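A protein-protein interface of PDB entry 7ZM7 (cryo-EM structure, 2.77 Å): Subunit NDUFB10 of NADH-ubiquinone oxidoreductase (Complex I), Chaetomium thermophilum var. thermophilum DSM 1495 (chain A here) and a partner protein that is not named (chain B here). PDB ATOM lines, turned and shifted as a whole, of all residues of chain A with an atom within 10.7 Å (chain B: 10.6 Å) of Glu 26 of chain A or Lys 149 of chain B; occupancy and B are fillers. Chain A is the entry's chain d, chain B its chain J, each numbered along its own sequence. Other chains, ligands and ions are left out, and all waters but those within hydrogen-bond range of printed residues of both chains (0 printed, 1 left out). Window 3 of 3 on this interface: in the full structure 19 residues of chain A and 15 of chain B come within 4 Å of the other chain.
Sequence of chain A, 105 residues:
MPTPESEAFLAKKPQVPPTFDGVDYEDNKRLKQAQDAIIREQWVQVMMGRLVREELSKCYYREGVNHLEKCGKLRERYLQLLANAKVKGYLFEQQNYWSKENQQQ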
ATOM      1  N   PHE A  20     -38.456 -18.897   9.444  1.00  0.00           N
ATOM      2  CA  PHE A  20     -37.157 -18.348   9.126  1.00  0.00           C
ATOM      3  C   PHE A  20     -36.147 -19.436   8.828  1.00  0.00           C
ATOM      4  O   PHE A  20     -35.017 -19.117   8.449  1.00  0.00           O
ATOM      5  CB  PHE A  20     -36.654 -17.466  10.272  1.00  0.00           C
ATOM      6  CG  PHE A  20     -37.373 -16.171  10.374  1.00  0.00           C
ATOM      7  CD1 PHE A  20     -37.134 -15.164   9.463  1.00  0.00           C
ATOM      8  CD2 PHE A  20     -38.312 -15.964  11.346  1.00  0.00           C
ATOM      9  CE1 PHE A  20     -37.805 -13.981   9.545  1.00  0.00           C
ATOM     10  CE2 PHE A  20     -38.983 -14.780  11.414  1.00  0.00           C
ATOM     11  CZ  PHE A  20     -38.724 -13.795  10.515  1.00  0.00           C
ATOM     12  N   GLY A  22     -33.931 -21.770   6.907  1.00  0.00           N
ATOM     13  CA  GLY A  22     -33.440 -21.697   5.543  1.00  0.00           C
ATOM     14  C   GLY A  22     -33.749 -20.392   4.846  1.00  0.00           C
ATOM     15  O   GLY A  22     -34.007 -20.385   3.637  1.00  0.00           O
ATOM     16  N   VAL A  23     -33.730 -19.283   5.577  1.00  0.00           N
ATOM     17  CA  VAL A  23     -33.998 -17.965   5.012  1.00  0.00           C
ATOM     18  C   VAL A  23     -32.751 -17.119   5.191  1.00  0.00           C
ATOM     19  O   VAL A  23     -32.386 -16.778   6.323  1.00  0.00           O
ATOM     20  CB  VAL A  23     -35.203 -17.288   5.676  1.00  0.00           C
ATOM     21  CG1 VAL A  23     -35.381 -15.887   5.130  1.00  0.00           C
ATOM     22  CG2 VAL A  23     -36.458 -18.114   5.477  1.00  0.00           C
ATOM     23  N   ASP A  24     -32.103 -16.775   4.084  1.00  0.00           N
ATOM     24  CA  ASP A  24     -30.942 -15.902   4.149  1.00  0.00           C
ATOM     25  C   ASP A  24     -31.374 -14.515   4.585  1.00  0.00           C
ATOM     26  O   ASP A  24     -32.283 -13.926   3.996  1.00  0.00           O
ATOM     27  CB  ASP A  24     -30.244 -15.831   2.797  1.00  0.00           C
ATOM     28  CG  ASP A  24     -29.036 -14.931   2.821  1.00  0.00           C
ATOM     29  OD1 ASP A  24     -28.002 -15.345   3.378  1.00  0.00           O
ATOM     30  OD2 ASP A  24     -29.119 -13.807   2.291  1.00  0.00           O
ATOM     31  N   TYR A  25     -30.745 -14.001   5.639  1.00  0.00           N
ATOM     32  CA  TYR A  25     -31.163 -12.709   6.159  1.00  0.00           C
ATOM     33  C   TYR A  25     -30.642 -11.561   5.309  1.00  0.00           C
ATOM     34  O   TYR A  25     -31.330 -10.548   5.161  1.00  0.00           O
ATOM     35  CB  TYR A  25     -30.721 -12.550   7.611  1.00  0.00           C
ATOM     36  CG  TYR A  25     -31.618 -13.268   8.581  1.00  0.00           C
ATOM     37  CD1 TYR A  25     -32.452 -14.276   8.155  1.00  0.00           C
ATOM     38  CD2 TYR A  25     -31.615 -12.962   9.918  1.00  0.00           C
ATOM     39  CE1 TYR A  25     -33.257 -14.944   9.025  1.00  0.00           C
ATOM     40  CE2 TYR A  25     -32.428 -13.631  10.798  1.00  0.00           C
ATOM     41  CZ  TYR A  25     -33.244 -14.621  10.342  1.00  0.00           C
ATOM     42  OH  TYR A  25     -34.063 -15.300  11.195  1.00  0.00           O
ATOM     43  N   GLU A  26     -29.465 -11.708   4.714  1.00  0.00           N
ATOM     44  CA  GLU A  26     -28.960 -10.669   3.832  1.00  0.00           C
ATOM     45  C   GLU A  26     -29.779 -10.540   2.556  1.00  0.00           C
ATOM     46  O   GLU A  26     -29.606  -9.561   1.823  1.00  0.00           O
ATOM     47  CB  GLU A  26     -27.500 -10.941   3.512  1.00  0.00           C
ATOM     48  CG  GLU A  26     -26.607 -10.822   4.723  1.00  0.00           C
ATOM     49  CD  GLU A  26     -25.155 -11.027   4.393  1.00  0.00           C
ATOM     50  OE1 GLU A  26     -24.855 -11.365   3.229  1.00  0.00           O
ATOM     51  OE2 GLU A  26     -24.309 -10.860   5.295  1.00  0.00           O
ATOM     52  N   ASP A  27     -30.682 -11.504   2.317  1.00  0.00           N
ATOM     53  CA  ASP A  27     -31.643 -11.348   1.203  1.00  0.00           C
ATOM     54  C   ASP A  27     -32.810 -10.642   1.862  1.00  0.00           C
ATOM     55  O   ASP A  27     -33.616 -11.330   2.490  1.00  0.00           O
ATOM     56  CB  ASP A  27     -32.149 -12.692   0.688  1.00  0.00           C
ATOM     57  CG  ASP A  27     -33.058 -12.584  -0.525  1.00  0.00           C
ATOM     58  OD1 ASP A  27     -33.290 -11.452  -0.994  1.00  0.00           O
ATOM     59  OD2 ASP A  27     -33.527 -13.636  -0.995  1.00  0.00           O
ATOM     60  N   ASN A  28     -32.917  -9.340   1.658  1.00  0.00           N
ATOM     61  CA  ASN A  28     -33.943  -8.535   2.349  1.00  0.00           C
ATOM     62  C   ASN A  28     -35.354  -8.890   1.897  1.00  0.00           C
ATOM     63  O   ASN A  28     -36.222  -8.968   2.757  1.00  0.00           O
ATOM     64  CB  ASN A  28     -33.610  -7.051   2.198  1.00  0.00           C
ATOM     65  CG  ASN A  28     -32.155  -6.741   2.475  1.00  0.00           C
ATOM     66  OD1 ASN A  28     -31.375  -6.549   1.548  1.00  0.00           O
ATOM     67  ND2 ASN A  28     -31.782  -6.697   3.743  1.00  0.00           N
ATOM     68  N   LYS A  29     -35.583  -9.087   0.597  1.00  0.00           N
ATOM     69  CA  LYS A  29     -36.972  -9.305   0.120  1.00  0.00           C
ATOM     70  C   LYS A  29     -37.534 -10.584   0.739  1.00  0.00           C
ATOM     71  O   LYS A  29     -38.670 -10.548   1.217  1.00  0.00           O
ATOM     72  CB  LYS A  29     -36.993  -9.377  -1.404  1.00  0.00           C
ATOM     73  CG  LYS A  29     -38.359  -9.640  -2.022  1.00  0.00           C
ATOM     74  CD  LYS A  29     -38.339  -9.682  -3.535  1.00  0.00           C
ATOM     75  CE  LYS A  29     -39.701  -9.957  -4.136  1.00  0.00           C
ATOM     76  NZ  LYS A  29     -39.649  -9.993  -5.616  1.00  0.00           N
ATOM     77  N   ARG A  30     -36.744 -11.654   0.760  1.00  0.00           N
ATOM     78  CA  ARG A  30     -37.169 -12.940   1.354  1.00  0.00           C
ATOM     79  C   ARG A  30     -37.381 -12.759   2.850  1.00  0.00           C
ATOM     80  O   ARG A  30     -38.365 -13.301   3.363  1.00  0.00           O
ATOM     81  CB  ARG A  30     -36.105 -13.995   1.048  1.00  0.00           C
ATOM     82  CG  ARG A  30     -36.459 -15.406   1.491  1.00  0.00           C
ATOM     83  CD  ARG A  30     -37.725 -15.912   0.828  1.00  0.00           C
ATOM     84  NE  ARG A  30     -38.276 -17.056   1.538  1.00  0.00           N
ATOM     85  CZ  ARG A  30     -39.135 -16.967   2.546  1.00  0.00           C
ATOM     86  NH1 ARG A  30     -39.545 -15.781   2.961  1.00  0.00           N
ATOM     87  NH2 ARG A  30     -39.587 -18.061   3.132  1.00  0.00           N
ATOM     88  N   LEU A  31     -36.483 -12.041   3.514  1.00  0.00           N
ATOM     89  CA  LEU A  31     -36.576 -11.866   4.986  1.00  0.00           C
ATOM     90  C   LEU A  31     -37.838 -11.079   5.341  1.00  0.00           C
ATOM     91  O   LEU A  31     -38.505 -11.478   6.291  1.00  0.00           O
ATOM     92  CB  LEU A  31     -35.314 -11.147   5.464  1.00  0.00           C
ATOM     93  CG  LEU A  31     -35.436 -10.478   6.833  1.00  0.00           C
ATOM     94  CD1 LEU A  31     -34.868 -11.360   7.933  1.00  0.00           C
ATOM     95  CD2 LEU A  31     -34.771  -9.114   6.840  1.00  0.00           C
ATOM     96  N   LYS A  32     -38.129 -10.013   4.594  1.00  0.00           N
ATOM     97  CA  LYS A  32     -39.299  -9.140   4.842  1.00  0.00           C
ATOM     98  C   LYS A  32     -40.573  -9.930   4.586  1.00  0.00           C
ATOM     99  O   LYS A  32     -41.549  -9.721   5.314  1.00  0.00           O
ATOM    100  CB  LYS A  32     -39.205  -7.866   4.003  1.00  0.00           C
ATOM    101  CG  LYS A  32     -38.079  -6.918   4.388  1.00  0.00           C
ATOM    102  CD  LYS A  32     -38.372  -6.088   5.612  1.00  0.00           C
ATOM    103  CE  LYS A  32     -39.369  -4.986   5.336  1.00  0.00           C
ATOM    104  NZ  LYS A  32     -39.775  -4.288   6.577  1.00  0.00           N
ATOM    105  N   ALA A  34     -40.758 -13.247   4.827  1.00  0.00           N
ATOM    106  CA  ALA A  34     -40.926 -14.116   5.977  1.00  0.00           C
ATOM    107  C   ALA A  34     -41.634 -13.383   7.095  1.00  0.00           C
ATOM    108  O   ALA A  34     -42.672 -13.833   7.576  1.00  0.00           O
ATOM    109  CB  ALA A  34     -39.571 -14.630   6.448  1.00  0.00           C
ATOM    110  N   GLN A  35     -41.117 -12.209   7.476  1.00  0.00           N
ATOM    111  CA  GLN A  35     -41.724 -11.443   8.561  1.00  0.00           C
ATOM    112  C   GLN A  35     -43.205 -11.237   8.309  1.00  0.00           C
ATOM    113  O   GLN A  35     -44.029 -11.473   9.194  1.00  0.00           O
ATOM    114  CB  GLN A  35     -41.036 -10.091   8.717  1.00  0.00           C
ATOM    115  CG  GLN A  35     -39.604 -10.124   9.160  1.00  0.00           C
ATOM    116  CD  GLN A  35     -38.903  -8.832   8.854  1.00  0.00           C
ATOM    117  OE1 GLN A  35     -39.416  -8.013   8.116  1.00  0.00           O
ATOM    118  NE2 GLN A  35     -37.736  -8.638   9.423  1.00  0.00           N
ATOM    119  N   GLN A  94     -37.406 -14.367  14.718  1.00  0.00           N
ATOM    120  CA  GLN A  94     -36.336 -13.962  13.813  1.00  0.00           C
ATOM    121  C   GLN A  94     -34.973 -14.133  14.454  1.00  0.00           C
ATOM    122  O   GLN A  94     -34.003 -14.460  13.771  1.00  0.00           O
ATOM    123  CB  GLN A  94     -36.530 -12.516  13.373  1.00  0.00           C
ATOM    124  CG  GLN A  94     -35.670 -12.123  12.205  1.00  0.00           C
ATOM    125  CD  GLN A  94     -35.961 -10.746  11.706  1.00  0.00           C
ATOM    126  OE1 GLN A  94     -36.888 -10.544  10.939  1.00  0.00           O
ATOM    127  NE2 GLN A  94     -35.165  -9.785  12.122  1.00  0.00           N
ATOM    128  N   GLN A  95     -34.884 -13.917  15.759  1.00  0.00           N
ATOM    129  CA  GLN A  95     -33.620 -13.850  16.467  1.00  0.00           C
ATOM    130  C   GLN A  95     -33.272 -15.116  17.214  1.00  0.00           C
ATOM    131  O   GLN A  95     -32.232 -15.151  17.868  1.00  0.00           O
ATOM    132  CB  GLN A  95     -33.640 -12.710  17.464  1.00  0.00           C
ATOM    133  CG  GLN A  95     -33.809 -11.355  16.890  1.00  0.00           C
ATOM    134  CD  GLN A  95     -33.944 -10.343  17.971  1.00  0.00           C
ATOM    135  OE1 GLN A  95     -33.864 -10.677  19.147  1.00  0.00           O
ATOM    136  NE2 GLN A  95     -34.160  -9.099  17.596  1.00  0.00           N
ATOM    137  N   TYR A  97     -33.365 -19.551  16.826  1.00  0.00           N
ATOM    138  CA  TYR A  97     -33.723 -20.788  16.140  1.00  0.00           C
ATOM    139  C   TYR A  97     -34.024 -21.874  17.157  1.00  0.00           C
ATOM    140  O   TYR A  97     -33.271 -22.074  18.110  1.00  0.00           O
ATOM    141  CB  TYR A  97     -32.644 -21.226  15.142  1.00  0.00           C
ATOM    142  CG  TYR A  97     -31.305 -21.550  15.727  1.00  0.00           C
ATOM    143  CD1 TYR A  97     -31.002 -22.823  16.180  1.00  0.00           C
ATOM    144  CD2 TYR A  97     -30.346 -20.565  15.857  1.00  0.00           C
ATOM    145  CE1 TYR A  97     -29.769 -23.105  16.734  1.00  0.00           C
ATOM    146  CE2 TYR A  97     -29.109 -20.837  16.398  1.00  0.00           C
ATOM    147  CZ  TYR A  97     -28.827 -22.104  16.841  1.00  0.00           C
ATOM    148  OH  TYR A  97     -27.593 -22.371  17.383  1.00  0.00           O
ATOM    149  N   ASP B 139      -8.231 -10.833  15.965  1.00  0.00           N
ATOM    150  CA  ASP B 139      -8.625 -10.155  14.703  1.00  0.00           C
ATOM    151  C   ASP B 139      -9.892  -9.330  14.911  1.00  0.00           C
ATOM    152  O   ASP B 139     -10.945  -9.930  15.133  1.00  0.00           O
ATOM    153  CB  ASP B 139      -8.903 -11.151  13.585  1.00  0.00           C
ATOM    154  CG  ASP B 139      -9.254 -10.431  12.301  1.00  0.00           C
ATOM    155  OD1 ASP B 139      -8.655  -9.367  12.040  1.00  0.00           O
ATOM    156  OD2 ASP B 139     -10.143 -10.912  11.603  1.00  0.00           O
ATOM    157  N   GLU B 140      -9.780  -8.010  14.814  1.00  0.00           N
ATOM    158  CA  GLU B 140     -10.946  -7.104  14.983  1.00  0.00           C
ATOM    159  C   GLU B 140     -11.961  -7.281  13.854  1.00  0.00           C
ATOM    160  O   GLU B 140     -13.143  -7.167  14.135  1.00  0.00           O
ATOM    161  CB  GLU B 140     -10.503  -5.664  15.249  1.00  0.00           C
ATOM    162  CG  GLU B 140     -10.321  -5.360  16.722  1.00  0.00           C
ATOM    163  CD  GLU B 140     -11.578  -5.495  17.567  1.00  0.00           C
ATOM    164  OE1 GLU B 140     -12.686  -5.318  17.020  1.00  0.00           O
ATOM    165  OE2 GLU B 140     -11.444  -5.780  18.773  1.00  0.00           O
ATOM    166  N   TYR B 141     -11.509  -7.538  12.630  1.00  0.00           N
ATOM    167  CA  TYR B 141     -12.437  -7.752  11.490  1.00  0.00           C
ATOM    168  C   TYR B 141     -13.297  -8.976  11.759  1.00  0.00           C
ATOM    169  O   TYR B 141     -14.513  -8.903  11.575  1.00  0.00           O
ATOM    170  CB  TYR B 141     -11.695  -7.878  10.164  1.00  0.00           C
ATOM    171  CG  TYR B 141     -12.536  -8.227   8.965  1.00  0.00           C
ATOM    172  CD1 TYR B 141     -13.134  -7.244   8.194  1.00  0.00           C
ATOM    173  CD2 TYR B 141     -12.724  -9.545   8.591  1.00  0.00           C
ATOM    174  CE1 TYR B 141     -13.904  -7.565   7.089  1.00  0.00           C
ATOM    175  CE2 TYR B 141     -13.482  -9.883   7.487  1.00  0.00           C
ATOM    176  CZ  TYR B 141     -14.074  -8.890   6.733  1.00  0.00           C
ATOM    177  OH  TYR B 141     -14.824  -9.242   5.651  1.00  0.00           O
ATOM    178  N   GLU B 142     -12.693 -10.050  12.251  1.00  0.00           N
ATOM    179  CA  GLU B 142     -13.509 -11.234  12.620  1.00  0.00           C
ATOM    180  C   GLU B 142     -14.448 -10.903  13.783  1.00  0.00           C
ATOM    181  O   GLU B 142     -15.612 -11.312  13.712  1.00  0.00           O
ATOM    182  CB  GLU B 142     -12.620 -12.444  12.891  1.00  0.00           C
ATOM    183  CG  GLU B 142     -12.379 -13.283  11.652  1.00  0.00           C
ATOM    184  CD  GLU B 142     -11.293 -14.333  11.797  1.00  0.00           C
ATOM    185  OE1 GLU B 142     -11.053 -15.070  10.822  1.00  0.00           O
ATOM    186  OE2 GLU B 142     -10.688 -14.408  12.885  1.00  0.00           O
ATOM    187  N   ARG B 143     -13.963 -10.198  14.807  1.00  0.00           N
ATOM    188  CA  ARG B 143     -14.801  -9.945  16.012  1.00  0.00           C
ATOM    189  C   ARG B 143     -15.999  -9.062  15.655  1.00  0.00           C
ATOM    190  O   ARG B 143     -17.123  -9.404  16.053  1.00  0.00           O
ATOM    191  CB  ARG B 143     -13.947  -9.328  17.121  1.00  0.00           C
ATOM    192  CG  ARG B 143     -14.739  -8.825  18.317  1.00  0.00           C
ATOM    193  CD  ARG B 143     -13.830  -8.265  19.391  1.00  0.00           C
ATOM    194  NE  ARG B 143     -14.571  -7.564  20.427  1.00  0.00           N
ATOM    195  CZ  ARG B 143     -15.026  -8.125  21.542  1.00  0.00           C
ATOM    196  NH1 ARG B 143     -14.816  -9.410  21.771  1.00  0.00           N
ATOM    197  NH2 ARG B 143     -15.689  -7.398  22.423  1.00  0.00           N
ATOM    198  N   LYS B 144     -15.759  -7.990  14.896  1.00  0.00           N
ATOM    199  CA  LYS B 144     -16.836  -7.054  14.502  1.00  0.00           C
ATOM    200  C   LYS B 144     -17.798  -7.756  13.552  1.00  0.00           C
ATOM    201  O   LYS B 144     -19.010  -7.624  13.752  1.00  0.00           O
ATOM    202  CB  LYS B 144     -16.213  -5.785  13.921  1.00  0.00           C
ATOM    203  CG  LYS B 144     -15.831  -4.711  14.930  1.00  0.00           C
ATOM    204  CD  LYS B 144     -17.032  -4.023  15.540  1.00  0.00           C
ATOM    205  CE  LYS B 144     -16.679  -2.733  16.249  1.00  0.00           C
ATOM    206  NZ  LYS B 144     -15.692  -2.948  17.332  1.00  0.00           N
ATOM    207  N   GLU B 145     -17.270  -8.498  12.582  1.00  0.00           N
ATOM    208  CA  GLU B 145     -18.127  -9.163  11.566  1.00  0.00           C
ATOM    209  C   GLU B 145     -18.987 -10.257  12.201  1.00  0.00           C
ATOM    210  O   GLU B 145     -20.125 -10.440  11.751  1.00  0.00           O
ATOM    211  CB  GLU B 145     -17.317  -9.611  10.351  1.00  0.00           C
ATOM    212  CG  GLU B 145     -16.945  -8.481   9.411  1.00  0.00           C
ATOM    213  CD  GLU B 145     -18.078  -7.982   8.536  1.00  0.00           C
ATOM    214  OE1 GLU B 145     -18.317  -8.595   7.483  1.00  0.00           O
ATOM    215  OE2 GLU B 145     -18.720  -6.986   8.907  1.00  0.00           O
ATOM    216  N   PHE B 146     -18.451 -10.981  13.181  1.00  0.00           N
ATOM    217  CA  PHE B 146     -19.261 -12.004  13.883  1.00  0.00           C
ATOM    218  C   PHE B 146     -20.428 -11.340  14.599  1.00  0.00           C
ATOM    219  O   PHE B 146     -21.537 -11.864  14.527  1.00  0.00           O
ATOM    220  CB  PHE B 146     -18.445 -12.783  14.914  1.00  0.00           C
ATOM    221  CG  PHE B 146     -19.278 -13.716  15.753  1.00  0.00           C
ATOM    222  CD1 PHE B 146     -19.826 -14.863  15.202  1.00  0.00           C
ATOM    223  CD2 PHE B 146     -19.543 -13.435  17.083  1.00  0.00           C
ATOM    224  CE1 PHE B 146     -20.611 -15.713  15.964  1.00  0.00           C
ATOM    225  CE2 PHE B 146     -20.330 -14.283  17.842  1.00  0.00           C
ATOM    226  CZ  PHE B 146     -20.860 -15.422  17.284  1.00  0.00           C
ATOM    227  N   LEU B 147     -20.186 -10.208  15.249  1.00  0.00           N
ATOM    228  CA  LEU B 147     -21.268  -9.599  16.052  1.00  0.00           C
ATOM    229  C   LEU B 147     -22.268  -8.877  15.142  1.00  0.00           C
ATOM    230  O   LEU B 147     -23.339  -8.542  15.633  1.00  0.00           O
ATOM    231  CB  LEU B 147     -20.623  -8.692  17.102  1.00  0.00           C
ATOM    232  CG  LEU B 147     -19.901  -9.407  18.238  1.00  0.00           C
ATOM    233  CD1 LEU B 147     -19.277  -8.400  19.185  1.00  0.00           C
ATOM    234  CD2 LEU B 147     -20.855 -10.318  18.988  1.00  0.00           C
ATOM    235  N   ARG B 148     -21.944  -8.672  13.867  1.00  0.00           N
ATOM    236  CA  ARG B 148     -22.891  -8.055  12.900  1.00  0.00           C
ATOM    237  C   ARG B 148     -23.757  -9.143  12.246  1.00  0.00           C
ATOM    238  O   ARG B 148     -24.948  -8.890  12.013  1.00  0.00           O
ATOM    239  CB  ARG B 148     -22.106  -7.295  11.821  1.00  0.00           C
ATOM    240  CG  ARG B 148     -22.978  -6.730  10.706  1.00  0.00           C
ATOM    241  CD  ARG B 148     -22.247  -5.992   9.603  1.00  0.00           C
ATOM    242  NE  ARG B 148     -21.518  -6.833   8.666  1.00  0.00           N
ATOM    243  CZ  ARG B 148     -22.017  -7.307   7.532  1.00  0.00           C
ATOM    244  NH1 ARG B 148     -21.271  -8.059   6.744  1.00  0.00           N
ATOM    245  NH2 ARG B 148     -23.260  -7.031   7.187  1.00  0.00           N
ATOM    246  N   LYS B 149     -23.180 -10.305  11.958  1.00  0.00           N
ATOM    247  CA  LYS B 149     -23.906 -11.389  11.321  1.00  0.00           C
ATOM    248  C   LYS B 149     -24.366 -12.461  12.293  1.00  0.00           C
ATOM    249  O   LYS B 149     -24.792 -13.530  11.856  1.00  0.00           O
ATOM    250  CB  LYS B 149     -23.063 -11.994  10.208  1.00  0.00           C
ATOM    251  CG  LYS B 149     -22.816 -11.035   9.080  1.00  0.00           C
ATOM    252  CD  LYS B 149     -22.086 -11.712   7.939  1.00  0.00           C
ATOM    253  CE  LYS B 149     -20.645 -12.022   8.278  1.00  0.00           C
ATOM    254  NZ  LYS B 149     -19.849 -10.799   8.422  1.00  0.00           N
ATOM    255  N   ASN B 150     -24.317 -12.195  13.592  1.00  0.00           N
ATOM    256  CA  ASN B 150     -24.812 -13.133  14.598  1.00  0.00           C
ATOM    257  C   ASN B 150     -26.302 -12.911  14.850  1.00  0.00           C
ATOM    258  O   ASN B 150     -26.757 -12.667  15.961  1.00  0.00           O
ATOM    259  CB  ASN B 150     -24.007 -12.992  15.878  1.00  0.00           C
ATOM    260  CG  ASN B 150     -24.359 -14.025  16.890  1.00  0.00           C
ATOM    261  OD1 ASN B 150     -24.824 -15.104  16.547  1.00  0.00           O
ATOM    262  ND2 ASN B 150     -24.152 -13.702  18.163  1.00  0.00           N
ATOM    263  N   ARG B 151     -27.067 -13.017  13.773  1.00  0.00           N
ATOM    264  CA  ARG B 151     -28.442 -12.544  13.781  1.00  0.00           C
ATOM    265  C   ARG B 151     -29.378 -13.471  14.545  1.00  0.00           C
ATOM    266  O   ARG B 151     -30.364 -13.001  15.120  1.00  0.00           O
ATOM    267  CB  ARG B 151     -28.906 -12.349  12.343  1.00  0.00           C
ATOM    268  CG  ARG B 151     -27.931 -11.546  11.515  1.00  0.00           C
ATOM    269  CD  ARG B 151     -28.655 -10.623  10.559  1.00  0.00           C
ATOM    270  NE  ARG B 151     -27.827  -9.531  10.051  1.00  0.00           N
ATOM    271  CZ  ARG B 151     -27.155  -9.552   8.901  1.00  0.00           C
ATOM    272  NH1 ARG B 151     -26.452  -8.497   8.530  1.00  0.00           N
ATOM    273  NH2 ARG B 151     -27.175 -10.616   8.123  1.00  0.00           N
ATOM    274  N   ARG B 152     -29.155 -14.784  14.466  1.00  0.00           N
ATOM    275  CA  ARG B 152     -30.033 -15.669  15.262  1.00  0.00           C
ATOM    276  C   ARG B 152     -29.217 -16.376  16.320  1.00  0.00           C
ATOM    277  O   ARG B 152     -28.014 -16.564  16.104  1.00  0.00           O
ATOM    278  CB  ARG B 152     -30.786 -16.715  14.444  1.00  0.00           C
ATOM    279  CG  ARG B 152     -31.371 -16.244  13.128  1.00  0.00           C
ATOM    280  CD  ARG B 152     -32.041 -17.456  12.511  1.00  0.00           C
ATOM    281  NE  ARG B 152     -33.259 -17.850  13.202  1.00  0.00           N
ATOM    282  CZ  ARG B 152     -34.088 -18.794  12.775  1.00  0.00           C
ATOM    283  NH1 ARG B 152     -33.817 -19.453  11.662  1.00  0.00           N
ATOM    284  NH2 ARG B 152     -35.180 -19.085  13.458  1.00  0.00           N
ATOM    285  N   ARG B 153     -29.908 -16.756  17.385  1.00  0.00           N
ATOM    286  CA  ARG B 153     -29.228 -17.414  18.511  1.00  0.00           C
ATOM    287  C   ARG B 153     -29.971 -18.703  18.876  1.00  0.00           C
ATOM    288  O   ARG B 153     -31.118 -18.842  18.468  1.00  0.00           O
ATOM    289  CB  ARG B 153     -29.077 -16.455  19.696  1.00  0.00           C
ATOM    290  CG  ARG B 153     -28.042 -15.362  19.480  1.00  0.00           C
ATOM    291  CD  ARG B 153     -28.100 -14.353  20.609  1.00  0.00           C
ATOM    292  NE  ARG B 153     -26.925 -13.500  20.666  1.00  0.00           N
ATOM    293  CZ  ARG B 153     -26.850 -12.308  20.095  1.00  0.00           C
ATOM    294  NH1 ARG B 153     -25.742 -11.597  20.185  1.00  0.00           N
ATOM    295  NH2 ARG B 153     -27.884 -11.839  19.422  1.00  0.00           N
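The guanidinium group (NH1) of Arg 152 of chain B lies within hydrogen-bond range of the backbone carbonyl oxygen (O) of Phe 20 of chain A, at 3.4 Å.
The side-chain hydroxyl of Tyr 25 of chain A sits close to the guanidinium group of Arg 152 of chain B (3.3 Å).
N of Arg 153 of chain B is in hydrogen-bond range of O of Gln 95 of chain A, 2.9 Å away.
The backbone NH (N) of Tyr 97 of chain A is in hydrogen-bond range of the backbone carbonyl oxygen (O) of Arg 153 of chain B (2.9 Å).
The side-chain carboxylate of Glu 145 of chain B lies within salt-bridge range of the side-chain amino group of Lys 149 of chain B.
The side-chain amide nitrogen (ND2) of Asn 150 of chain B lies close to the guanidinium group (NH1) of Arg 153 of chain B (3.3 Å).
The side-chain carboxylate (OD2) of Asp 24 of chain A is in hydrogen-bond range of the backbone NH (N) of Glu 26 of chain A, 3.2 Å away.
The side-chain hydroxyl (OH) of Tyr 25 of chain A is in hydrogen-bond range of the backbone carbonyl oxygen (O) of Gln 94 of chain A.
The side-chain amide nitrogen (NE2) of Gln 35 of chain A sits at hydrogen-bond distance from the side-chain amide oxygen (OE1) of Gln 94 of chain A.
Tyr 25 of chain A touches Arg 151 of chain B (CD2 to CB, 3.7 Å).
Glu 26 of chain A touches Lys 149 of chain B.
CG of Glu 26 of chain A touches NH2 of Arg 151 of chain B, at 3.5 Å.
CG of Arg 152 of chain B touches O of Gln 94 of chain A (3.2 Å).
Gln 95 of chain A touches Arg 151 of chain B.
Gln 95 of chain A touches Arg 152 of chain B.
Arg 152 of chain B touches Tyr 97 of chain A.
Glu 26 of chain A touches two residues of chain B.
Arg 30 of chain A touches none of the printed residues of chain B.
Of the printed residues of chain B, Gln 94 of chain A touches Arg 152.
Tyr 141 of chain B touches none of the printed residues of chain A.
No residue of chain A comes within 4 Å of Glu 145 of chain B.
Lys 149 of chain B touches just one residue of chain A: Glu 26.
No residue of chain A comes within 4 Å of Asn 150 of chain B.
Of the printed residues of chain A, Arg 152 of chain B touches Phe 20, Tyr 25, Gln 94, Gln 95 and Tyr 97.
The nearest residue of chain B that does not touch Glu 26 of chain A is Arg 148 of chain B (4.4 Å).
The nearest residue of chain A that does not touch Lys 149 of chain B is Tyr 25 of chain A (7.1 Å).
The nearest printed residue of chain B that does not touch Tyr 97 of chain A is Asn 150 of chain B (7.2 Å).
Of the 17 printed residues of chain A, 6 touch a printed residue of chain B.
Hydrophobic or aromatic side chains of chain A within 4 Å of the printed part of chain B: Phe 20, Tyr 25 and Tyr 97.
Of the 15 printed residues of chain B, 4 touch a printed residue of chain A.
Along chain B the printed residues that touch a printed residue of chain A span positions 149 to 153.
Among the printed residues, 11 pairs touch across the chains.
Among the printed residues, no Asp or Glu carboxylate lies within 4 Å of a Lys or Arg side-chain nitrogen of the other chain.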
